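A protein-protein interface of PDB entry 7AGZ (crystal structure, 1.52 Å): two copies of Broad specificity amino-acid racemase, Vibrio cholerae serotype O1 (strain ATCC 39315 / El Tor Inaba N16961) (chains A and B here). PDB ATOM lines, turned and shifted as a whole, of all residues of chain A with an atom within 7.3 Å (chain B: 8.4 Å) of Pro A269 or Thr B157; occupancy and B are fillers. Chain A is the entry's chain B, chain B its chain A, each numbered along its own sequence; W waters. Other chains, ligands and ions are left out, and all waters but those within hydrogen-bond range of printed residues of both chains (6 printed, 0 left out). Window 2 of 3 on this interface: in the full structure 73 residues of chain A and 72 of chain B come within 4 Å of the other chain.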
ATOM      1  N   HIS A 266     -19.704 -22.055  31.789  1.00  0.00           N
ATOM      2  CA  HIS A 266     -20.697 -21.346  30.988  1.00  0.00           C
ATOM      3  C   HIS A 266     -21.428 -22.328  30.084  1.00  0.00           C
ATOM      4  O   HIS A 266     -20.792 -23.122  29.381  1.00  0.00           O
ATOM      5  CB  HIS A 266     -20.001 -20.272  30.133  1.00  0.00           C
ATOM      6  CG  HIS A 266     -19.211 -19.266  30.924  1.00  0.00           C
ATOM      7  ND1 HIS A 266     -19.611 -17.953  31.083  1.00  0.00           N
ATOM      8  CD2 HIS A 266     -18.036 -19.384  31.593  1.00  0.00           C
ATOM      9  CE1 HIS A 266     -18.709 -17.301  31.807  1.00  0.00           C
ATOM     10  NE2 HIS A 266     -17.750 -18.150  32.148  1.00  0.00           N
ATOM     11  N   HIS A 267     -22.757 -22.239  30.084  1.00  0.00           N
ATOM     12  CA  HIS A 267     -23.623 -23.044  29.221  1.00  0.00           C
ATOM     13  C   HIS A 267     -23.863 -22.308  27.913  1.00  0.00           C
ATOM     14  O   HIS A 267     -24.409 -21.191  27.913  1.00  0.00           O
ATOM     15  CB  HIS A 267     -24.915 -23.341  29.975  1.00  0.00           C
ATOM     16  CG  HIS A 267     -24.680 -24.233  31.162  1.00  0.00           C
ATOM     17  ND1 HIS A 267     -23.967 -23.806  32.268  1.00  0.00           N
ATOM     18  CD2 HIS A 267     -24.982 -25.534  31.395  1.00  0.00           C
ATOM     19  CE1 HIS A 267     -23.876 -24.792  33.144  1.00  0.00           C
ATOM     20  NE2 HIS A 267     -24.482 -25.850  32.639  1.00  0.00           N
ATOM     21  N   LEU A 268     -23.547 -22.967  26.805  1.00  0.00           N
ATOM     22  CA  LEU A 268     -23.690 -22.397  25.461  1.00  0.00           C
ATOM     23  C   LEU A 268     -24.472 -23.316  24.533  1.00  0.00           C
ATOM     24  O   LEU A 268     -24.243 -24.536  24.541  1.00  0.00           O
ATOM     25  CB  LEU A 268     -22.321 -22.134  24.836  1.00  0.00           C
ATOM     26  CG  LEU A 268     -21.592 -20.798  24.920  1.00  0.00           C
ATOM     27  CD1 LEU A 268     -20.512 -20.810  23.877  1.00  0.00           C
ATOM     28  CD2 LEU A 268     -22.496 -19.563  24.674  1.00  0.00           C
ATOM     29  N   PRO A 269     -25.493 -22.817  23.856  1.00  0.00           N
ATOM     30  CA  PRO A 269     -26.250 -23.675  22.945  1.00  0.00           C
ATOM     31  C   PRO A 269     -25.435 -24.017  21.708  1.00  0.00           C
ATOM     32  O   PRO A 269     -24.378 -23.449  21.448  1.00  0.00           O
ATOM     33  CB  PRO A 269     -27.466 -22.812  22.576  1.00  0.00           C
ATOM     34  CG  PRO A 269     -26.991 -21.375  22.781  1.00  0.00           C
ATOM     35  CD  PRO A 269     -25.960 -21.412  23.880  1.00  0.00           C
ATOM     36  N   LYS A 270     -25.904 -25.032  20.980  1.00  0.00           N
ATOM     37  CA  LYS A 270     -25.424 -25.378  19.642  1.00  0.00           C
ATOM     38  C   LYS A 270     -25.323 -24.113  18.767  1.00  0.00           C
ATOM     39  O   LYS A 270     -26.091 -23.160  18.928  1.00  0.00           O
ATOM     40  CB  LYS A 270     -26.307 -26.491  19.063  1.00  0.00           C
ATOM     41  CG  LYS A 270     -25.818 -27.230  17.853  1.00  0.00           C
ATOM     42  CD  LYS A 270     -27.021 -28.034  17.332  1.00  0.00           C
ATOM     43  CE  LYS A 270     -26.723 -29.087  16.248  1.00  0.00           C
ATOM     44  NZ  LYS A 270     -25.700 -28.797  15.212  1.00  0.00           N
ATOM     45  N   ASP A 271     -24.345 -24.058  17.856  1.00  0.00           N
ATOM     46  CA  ASP A 271     -24.146 -22.957  16.885  1.00  0.00           C
ATOM     47  C   ASP A 271     -23.737 -21.636  17.547  1.00  0.00           C
ATOM     48  O   ASP A 271     -24.111 -20.546  17.102  1.00  0.00           O
ATOM     49  CB  ASP A 271     -25.380 -22.721  16.009  1.00  0.00           C
ATOM     50  CG  ASP A 271     -25.768 -23.937  15.215  1.00  0.00           C
ATOM     51  OD1 ASP A 271     -24.872 -24.632  14.693  1.00  0.00           O
ATOM     52  OD2 ASP A 271     -26.985 -24.174  15.083  1.00  0.00           O
ATOM     53  N   SER A 272     -22.981 -21.721  18.632  1.00  0.00           N
ATOM     54  CA  SER A 272     -22.448 -20.518  19.240  1.00  0.00           C
ATOM     55  C   SER A 272     -20.968 -20.411  18.940  1.00  0.00           C
ATOM     56  O   SER A 272     -20.212 -21.366  19.133  1.00  0.00           O
ATOM     57  CB  SER A 272     -22.667 -20.525  20.758  1.00  0.00           C
ATOM     58  OG  SER A 272     -23.930 -21.060  21.102  1.00  0.00           O
ATOM     59  N   THR A 273     -20.581 -19.194  18.543  1.00  0.00           N
ATOM     60  CA  THR A 273     -19.188 -18.908  18.240  1.00  0.00           C
ATOM     61  C   THR A 273     -18.393 -18.669  19.524  1.00  0.00           C
ATOM     62  O   THR A 273     -18.919 -18.163  20.524  1.00  0.00           O
ATOM     63  CB  THR A 273     -19.135 -17.694  17.309  1.00  0.00           C
ATOM     64  OG1 THR A 273     -19.958 -16.667  17.879  1.00  0.00           O
ATOM     65  CG2 THR A 273     -19.751 -18.098  15.973  1.00  0.00           C
ATOM     66  N   THR A 281     -17.158 -22.963  16.454  1.00  0.00           N
ATOM     67  CA  THR A 281     -18.603 -22.847  16.644  1.00  0.00           C
ATOM     68  C   THR A 281     -19.099 -24.146  17.264  1.00  0.00           C
ATOM     69  O   THR A 281     -18.716 -25.228  16.800  1.00  0.00           O
ATOM     70  CB  THR A 281     -19.329 -22.558  15.314  1.00  0.00           C
ATOM     71  OG1 THR A 281     -18.855 -21.322  14.734  1.00  0.00           O
ATOM     72  CG2 THR A 281     -20.811 -22.431  15.558  1.00  0.00           C
ATOM     73  N   THR A 282     -19.855 -24.063  18.358  1.00  0.00           N
ATOM     74  CA  THR A 282     -20.335 -25.294  18.978  1.00  0.00           C
ATOM     75  C   THR A 282     -21.257 -26.045  18.015  1.00  0.00           C
ATOM     76  O   THR A 282     -22.069 -25.446  17.299  1.00  0.00           O
ATOM     77  CB  THR A 282     -21.096 -25.004  20.264  1.00  0.00           C
ATOM     78  OG1 THR A 282     -22.211 -24.128  19.996  1.00  0.00           O
ATOM     79  CG2 THR A 282     -20.175 -24.366  21.296  1.00  0.00           C
ATOM     80  N   SER A 283     -21.158 -27.369  18.044  1.00  0.00           N
ATOM     81  CA  SER A 283     -21.951 -28.293  17.245  1.00  0.00           C
ATOM     82  C   SER A 283     -23.025 -28.948  18.091  1.00  0.00           C
ATOM     83  O   SER A 283     -23.720 -29.838  17.598  1.00  0.00           O
ATOM     84  CB  SER A 283     -21.047 -29.337  16.569  1.00  0.00           C
ATOM     85  OG  SER A 283     -20.805 -30.455  17.401  1.00  0.00           O
ATOM     86  N   ARG A 284     -23.116 -28.578  19.372  1.00  0.00           N
ATOM     87  CA  ARG A 284     -23.962 -29.231  20.366  1.00  0.00           C
ATOM     88  C   ARG A 284     -24.090 -28.290  21.549  1.00  0.00           C
ATOM     89  O   ARG A 284     -23.268 -27.380  21.725  1.00  0.00           O
ATOM     90  CB  ARG A 284     -23.367 -30.560  20.848  1.00  0.00           C
ATOM     91  CG  ARG A 284     -22.005 -30.374  21.526  1.00  0.00           C
ATOM     92  CD  ARG A 284     -21.322 -31.664  21.993  1.00  0.00           C
ATOM     93  NE  ARG A 284     -19.975 -31.370  22.507  1.00  0.00           N
ATOM     94  CZ  ARG A 284     -19.085 -32.289  22.881  1.00  0.00           C
ATOM     95  NH1 ARG A 284     -19.384 -33.581  22.815  1.00  0.00           N
ATOM     96  NH2 ARG A 284     -17.893 -31.923  23.338  1.00  0.00           N
ATOM     97  N   ASP A 285     -25.113 -28.517  22.368  1.00  0.00           N
ATOM     98  CA  ASP A 285     -25.186 -27.793  23.629  1.00  0.00           C
ATOM     99  C   ASP A 285     -23.945 -28.131  24.452  1.00  0.00           C
ATOM    100  O   ASP A 285     -23.565 -29.297  24.590  1.00  0.00           O
ATOM    101  CB  ASP A 285     -26.457 -28.155  24.392  1.00  0.00           C
ATOM    102  CG  ASP A 285     -27.704 -27.597  23.725  1.00  0.00           C
ATOM    103  OD1 ASP A 285     -27.558 -26.819  22.758  1.00  0.00           O
ATOM    104  OD2 ASP A 285     -28.822 -27.924  24.172  1.00  0.00           O
ATOM    105  N   SER A 286     -23.284 -27.099  24.960  1.00  0.00           N
ATOM    106  CA  SER A 286     -21.929 -27.169  25.490  1.00  0.00           C
ATOM    107  C   SER A 286     -21.832 -26.656  26.925  1.00  0.00           C
ATOM    108  O   SER A 286     -22.659 -25.855  27.376  1.00  0.00           O
ATOM    109  CB  SER A 286     -20.992 -26.347  24.586  1.00  0.00           C
ATOM    110  OG  SER A 286     -20.734 -27.053  23.376  1.00  0.00           O
ATOM    111  N   ASN B 144     -23.888 -12.346  26.142  1.00  0.00           N
ATOM    112  CA  ASN B 144     -23.213 -12.955  24.964  1.00  0.00           C
ATOM    113  C   ASN B 144     -23.804 -12.519  23.612  1.00  0.00           C
ATOM    114  O   ASN B 144     -23.564 -13.168  22.697  1.00  0.00           O
ATOM    115  CB  ASN B 144     -23.237 -14.475  25.021  1.00  0.00           C
ATOM    116  CG  ASN B 144     -22.218 -15.127  24.124  1.00  0.00           C
ATOM    117  OD1 ASN B 144     -21.082 -14.733  24.094  1.00  0.00           O
ATOM    118  ND2 ASN B 144     -22.606 -16.197  23.463  1.00  0.00           N
ATOM    119  N   ILE B 153     -23.145 -14.439  29.659  1.00  0.00           N
ATOM    120  CA  ILE B 153     -24.334 -15.330  29.703  1.00  0.00           C
ATOM    121  C   ILE B 153     -25.064 -15.263  28.353  1.00  0.00           C
ATOM    122  O   ILE B 153     -25.456 -14.236  27.931  1.00  0.00           O
ATOM    123  CB  ILE B 153     -25.272 -15.022  30.894  1.00  0.00           C
ATOM    124  CG1 ILE B 153     -26.449 -15.996  30.928  1.00  0.00           C
ATOM    125  CG2 ILE B 153     -25.775 -13.602  30.884  1.00  0.00           C
ATOM    126  CD1 ILE B 153     -26.069 -17.428  31.302  1.00  0.00           C
ATOM    127  N   ASP B 154     -25.210 -16.407  27.730  1.00  0.00           N
ATOM    128  CA  ASP B 154     -25.943 -16.429  26.450  1.00  0.00           C
ATOM    129  C   ASP B 154     -27.435 -16.399  26.754  1.00  0.00           C
ATOM    130  O   ASP B 154     -27.821 -17.115  27.575  1.00  0.00           O
ATOM    131  CB  ASP B 154     -25.521 -17.617  25.600  1.00  0.00           C
ATOM    132  CG  ASP B 154     -26.189 -17.649  24.237  1.00  0.00           C
ATOM    133  OD1 ASP B 154     -27.299 -18.141  24.207  1.00  0.00           O
ATOM    134  OD2 ASP B 154     -25.566 -17.219  23.273  1.00  0.00           O
ATOM    135  N   MET B 155     -28.198 -15.565  26.061  1.00  0.00           N
ATOM    136  CA  MET B 155     -29.641 -15.415  26.325  1.00  0.00           C
ATOM    137  C   MET B 155     -30.457 -15.768  25.079  1.00  0.00           C
ATOM    138  O   MET B 155     -31.569 -15.360  25.026  1.00  0.00           O
ATOM    139  CB  MET B 155     -29.962 -13.999  26.755  1.00  0.00           C
ATOM    140  CG  MET B 155     -29.270 -13.628  28.057  1.00  0.00           C
ATOM    141  SD  MET B 155     -29.589 -12.011  28.559  1.00  0.00           S
ATOM    142  CE  MET B 155     -31.313 -11.838  28.097  1.00  0.00           C
ATOM    143  N   THR B 156     -29.944 -16.631  24.219  1.00  0.00           N
ATOM    144  CA  THR B 156     -30.704 -17.045  23.009  1.00  0.00           C
ATOM    145  C   THR B 156     -31.647 -18.207  23.318  1.00  0.00           C
ATOM    146  O   THR B 156     -32.346 -18.592  22.443  1.00  0.00           O
ATOM    147  CB  THR B 156     -29.799 -17.451  21.853  1.00  0.00           C
ATOM    148  OG1 THR B 156     -29.103 -18.626  22.214  1.00  0.00           O
ATOM    149  CG2 THR B 156     -28.808 -16.369  21.480  1.00  0.00           C
ATOM    150  N   THR B 157     -31.631 -18.710  24.531  1.00  0.00           N
ATOM    151  CA  THR B 157     -32.496 -19.824  24.979  1.00  0.00           C
ATOM    152  C   THR B 157     -33.187 -19.425  26.275  1.00  0.00           C
ATOM    153  O   THR B 157     -32.767 -18.514  26.917  1.00  0.00           O
ATOM    154  CB  THR B 157     -31.715 -21.119  25.190  1.00  0.00           C
ATOM    155  OG1 THR B 157     -30.862 -20.937  26.321  1.00  0.00           O
ATOM    156  CG2 THR B 157     -30.959 -21.593  23.970  1.00  0.00           C
ATOM    157  N   GLU B 158     -34.221 -20.162  26.636  1.00  0.00           N
ATOM    158  CA  GLU B 158     -34.955 -19.879  27.870  1.00  0.00           C
ATOM    159  C   GLU B 158     -34.046 -20.154  29.063  1.00  0.00           C
ATOM    160  O   GLU B 158     -34.144 -19.450  29.980  1.00  0.00           O
ATOM    161  CB  GLU B 158     -36.215 -20.731  27.952  1.00  0.00           C
ATOM    162  CG  GLU B 158     -37.300 -20.271  26.992  1.00  0.00           C
ATOM    163  CD  GLU B 158     -37.761 -18.839  27.116  1.00  0.00           C
ATOM    164  OE1 GLU B 158     -37.640 -18.091  26.142  1.00  0.00           O
ATOM    165  OE2 GLU B 158     -38.251 -18.489  28.181  1.00  0.00           O
ATOM    166  N   ALA B 159     -33.218 -21.180  28.976  1.00  0.00           N
ATOM    167  CA  ALA B 159     -32.286 -21.482  30.082  1.00  0.00           C
ATOM    168  C   ALA B 159     -31.379 -20.277  30.331  1.00  0.00           C
ATOM    169  O   ALA B 159     -31.142 -19.966  31.443  1.00  0.00           O
ATOM    170  CB  ALA B 159     -31.451 -22.686  29.737  1.00  0.00           C
ATOM    171  N   GLY B 160     -30.848 -19.718  29.262  1.00  0.00           N
ATOM    172  CA  GLY B 160     -29.958 -18.558  29.420  1.00  0.00           C
ATOM    173  C   GLY B 160     -30.656 -17.345  29.985  1.00  0.00           C
ATOM    174  O   GLY B 160     -30.134 -16.723  30.872  1.00  0.00           O
ATOM    175  N   LYS B 161     -31.857 -17.078  29.500  1.00  0.00           N
ATOM    176  CA  LYS B 161     -32.620 -15.942  30.023  1.00  0.00           C
ATOM    177  C   LYS B 161     -32.878 -16.130  31.519  1.00  0.00           C
ATOM    178  O   LYS B 161     -32.771 -15.193  32.235  1.00  0.00           O
ATOM    179  CB  LYS B 161     -33.901 -15.734  29.212  1.00  0.00           C
ATOM    180  CG  LYS B 161     -33.649 -15.263  27.800  1.00  0.00           C
ATOM    181  CD  LYS B 161     -34.919 -15.161  27.016  1.00  0.00           C
ATOM    182  CE  LYS B 161     -34.666 -14.670  25.605  1.00  0.00           C
ATOM    183  NZ  LYS B 161     -34.555 -15.778  24.624  1.00  0.00           N
ATOM    184  N   LYS B 162     -33.253 -17.327  31.926  1.00  0.00           N
ATOM    185  CA  LYS B 162     -33.537 -17.570  33.353  1.00  0.00           C
ATOM    186  C   LYS B 162     -32.238 -17.416  34.174  1.00  0.00           C
ATOM    187  O   LYS B 162     -32.309 -16.904  35.205  1.00  0.00           O
ATOM    188  CB  LYS B 162     -34.231 -18.930  33.536  1.00  0.00           C
ATOM    189  CG  LYS B 162     -35.743 -18.939  33.259  1.00  0.00           C
ATOM    190  CD  LYS B 162     -36.351 -20.330  33.312  1.00  0.00           C
ATOM    191  CE  LYS B 162     -37.881 -20.366  33.313  1.00  0.00           C
ATOM    192  NZ  LYS B 162     -38.508 -21.715  33.490  1.00  0.00           N
ATOM    193  N   GLU B 163     -31.109 -17.855  33.644  1.00  0.00           N
ATOM    194  CA  GLU B 163     -29.839 -17.717  34.397  1.00  0.00           C
ATOM    195  C   GLU B 163     -29.491 -16.228  34.463  1.00  0.00           C
ATOM    196  O   GLU B 163     -29.120 -15.782  35.453  1.00  0.00           O
ATOM    197  CB  GLU B 163     -28.724 -18.537  33.762  1.00  0.00           C
ATOM    198  CG  GLU B 163     -27.412 -18.438  34.559  1.00  0.00           C
ATOM    199  CD  GLU B 163     -26.334 -19.433  34.169  1.00  0.00           C
ATOM    200  OE1 GLU B 163     -25.305 -19.451  34.820  1.00  0.00           O
ATOM    201  OE2 GLU B 163     -26.544 -20.167  33.245  1.00  0.00           O
ATOM    202  N   ALA B 164     -29.695 -15.522  33.364  1.00  0.00           N
ATOM    203  CA  ALA B 164     -29.407 -14.081  33.395  1.00  0.00           C
ATOM    204  C   ALA B 164     -30.237 -13.363  34.464  1.00  0.00           C
ATOM    205  O   ALA B 164     -29.714 -12.532  35.177  1.00  0.00           O
ATOM    206  CB  ALA B 164     -29.613 -13.497  32.026  1.00  0.00           C
ATOM    207  N   TRP B 203     -34.591  -6.101  27.931  1.00  0.00           N
ATOM    208  CA  TRP B 203     -35.391  -7.169  28.520  1.00  0.00           C
ATOM    209  C   TRP B 203     -34.894  -7.514  29.919  1.00  0.00           C
ATOM    210  O   TRP B 203     -35.690  -7.660  30.848  1.00  0.00           O
ATOM    211  CB  TRP B 203     -35.370  -8.412  27.628  1.00  0.00           C
ATOM    212  CG  TRP B 203     -36.230  -9.528  28.175  1.00  0.00           C
ATOM    213  CD1 TRP B 203     -37.567  -9.691  27.982  1.00  0.00           C
ATOM    214  CD2 TRP B 203     -35.819 -10.585  29.043  1.00  0.00           C
ATOM    215  NE1 TRP B 203     -38.014 -10.815  28.644  1.00  0.00           N
ATOM    216  CE2 TRP B 203     -36.956 -11.375  29.310  1.00  0.00           C
ATOM    217  CE3 TRP B 203     -34.596 -10.956  29.607  1.00  0.00           C
ATOM    218  CZ2 TRP B 203     -36.904 -12.512  30.125  1.00  0.00           C
ATOM    219  CZ3 TRP B 203     -34.549 -12.088  30.419  1.00  0.00           C
ATOM    220  CH2 TRP B 203     -35.697 -12.852  30.662  1.00  0.00           C
HETATM  221  O   HOH W   1     -27.008 -20.313  28.267  1.00  0.00           O
HETATM  222  O   HOH W   2     -25.316 -18.425  20.801  1.00  0.00           O
HETATM  223  O   HOH W   3     -23.301 -21.575  34.626  1.00  0.00           O
HETATM  224  O   HOH W   4     -21.315 -17.273  21.309  1.00  0.00           O
HETATM  225  O   HOH W   5     -24.258 -20.580  31.835  1.00  0.00           O
HETATM  226  O   HOH W   6     -23.279 -18.624  28.460  1.00  0.00           O
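O of Ile B153 lies within hydrogen-bond range of N of Asn B144.
ND2 of Asn B144 lies within hydrogen-bond range of OD2 of Asp B154, at 3.1 Å.
The side-chain hydroxyl of Thr B156 lies within hydrogen-bond range of the side-chain carboxylate of Asp B154 (2.7 Å).
The backbone carbonyl oxygen of Leu A268 is in hydrogen-bond range of the backbone NH of Ser A286, at 2.8 Å.
OG of Ser A272 is in hydrogen-bond range of O of Pro A269 (2.5 Å).
OG1 of Thr A282 is in hydrogen-bond range of O of Pro A269, 2.7 Å away.
Asn B144 touches Leu A268 (ND2 to CD2, 3.6 Å).
Leu A268 touches Asp B154.
Asp B154 touches Pro A269.
OG1 of Thr B156 touches CG of Pro A269, 3.5 Å away.
Thr B157 touches Pro A269.
Of the printed residues of chain B, Pro A269 touches Asp B154 (3.5 Å), Thr B156 (3.5 Å) and Thr B157 (3.95 Å).
Of the printed residues of chain A, Thr B157 touches Pro A269 (3.95 Å).
Of the printed residues of chain A, Asp B154 touches Leu A268 (3.7 Å) and Pro A269 (3.5 Å).
Of the printed residues of chain B, Leu A268 touches Asn B144 and Asp B154.
Of the printed residues of chain A, Thr B156 touches Pro A269.
Of the printed residues of chain A, Asn B144 touches Leu A268.
Ala B164 touches none of the printed residues of chain A.
The nearest residue of chain A that does not touch Thr B157 is Asp A285 (6.4 Å).
Of the 14 printed residues of chain B, 4 touch a printed residue of chain A.
Printed residues of chain B that touch a printed residue of chain A: Asn B144, Asp B154, Thr B156 and Thr B157.
Of the 14 printed residues of chain A, 2 touch a printed residue of chain B.
Among the printed residues, no Asp or Glu carboxylate lies within 4 Å of a Lys or Arg side-chain nitrogen of the other chain.
No position is printed for both chains.
Water W4 lies within hydrogen-bond range of the backbone carbonyl oxygen (O) of Thr A273 and the side-chain amide nitrogen (ND2) of Asn B144.
Water W5 lies within hydrogen-bond range of the side-chain carboxylate (OE2) of Glu B163 (2.7 Å) and the backbone NH (N) of His A267 (2.8 Å).
Water W2 lies within hydrogen-bond range of OD2 of Asp B154 (2.8 Å) and OG of Ser A272 (3.0 Å).
Water W1 bridges the backbone carbonyl oxygen of His A267 and the backbone carbonyl oxygen of Asp B154.
Water W6 lies within hydrogen-bond range of O of His A267 (2.9 Å) and N of Asp B154 (3.0 Å).
Water W3 bridges the side-chain carboxylate (OE1) of Glu B163 (2.9 Å) and a ring nitrogen (ND1) of His A267 (3.3 Å).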
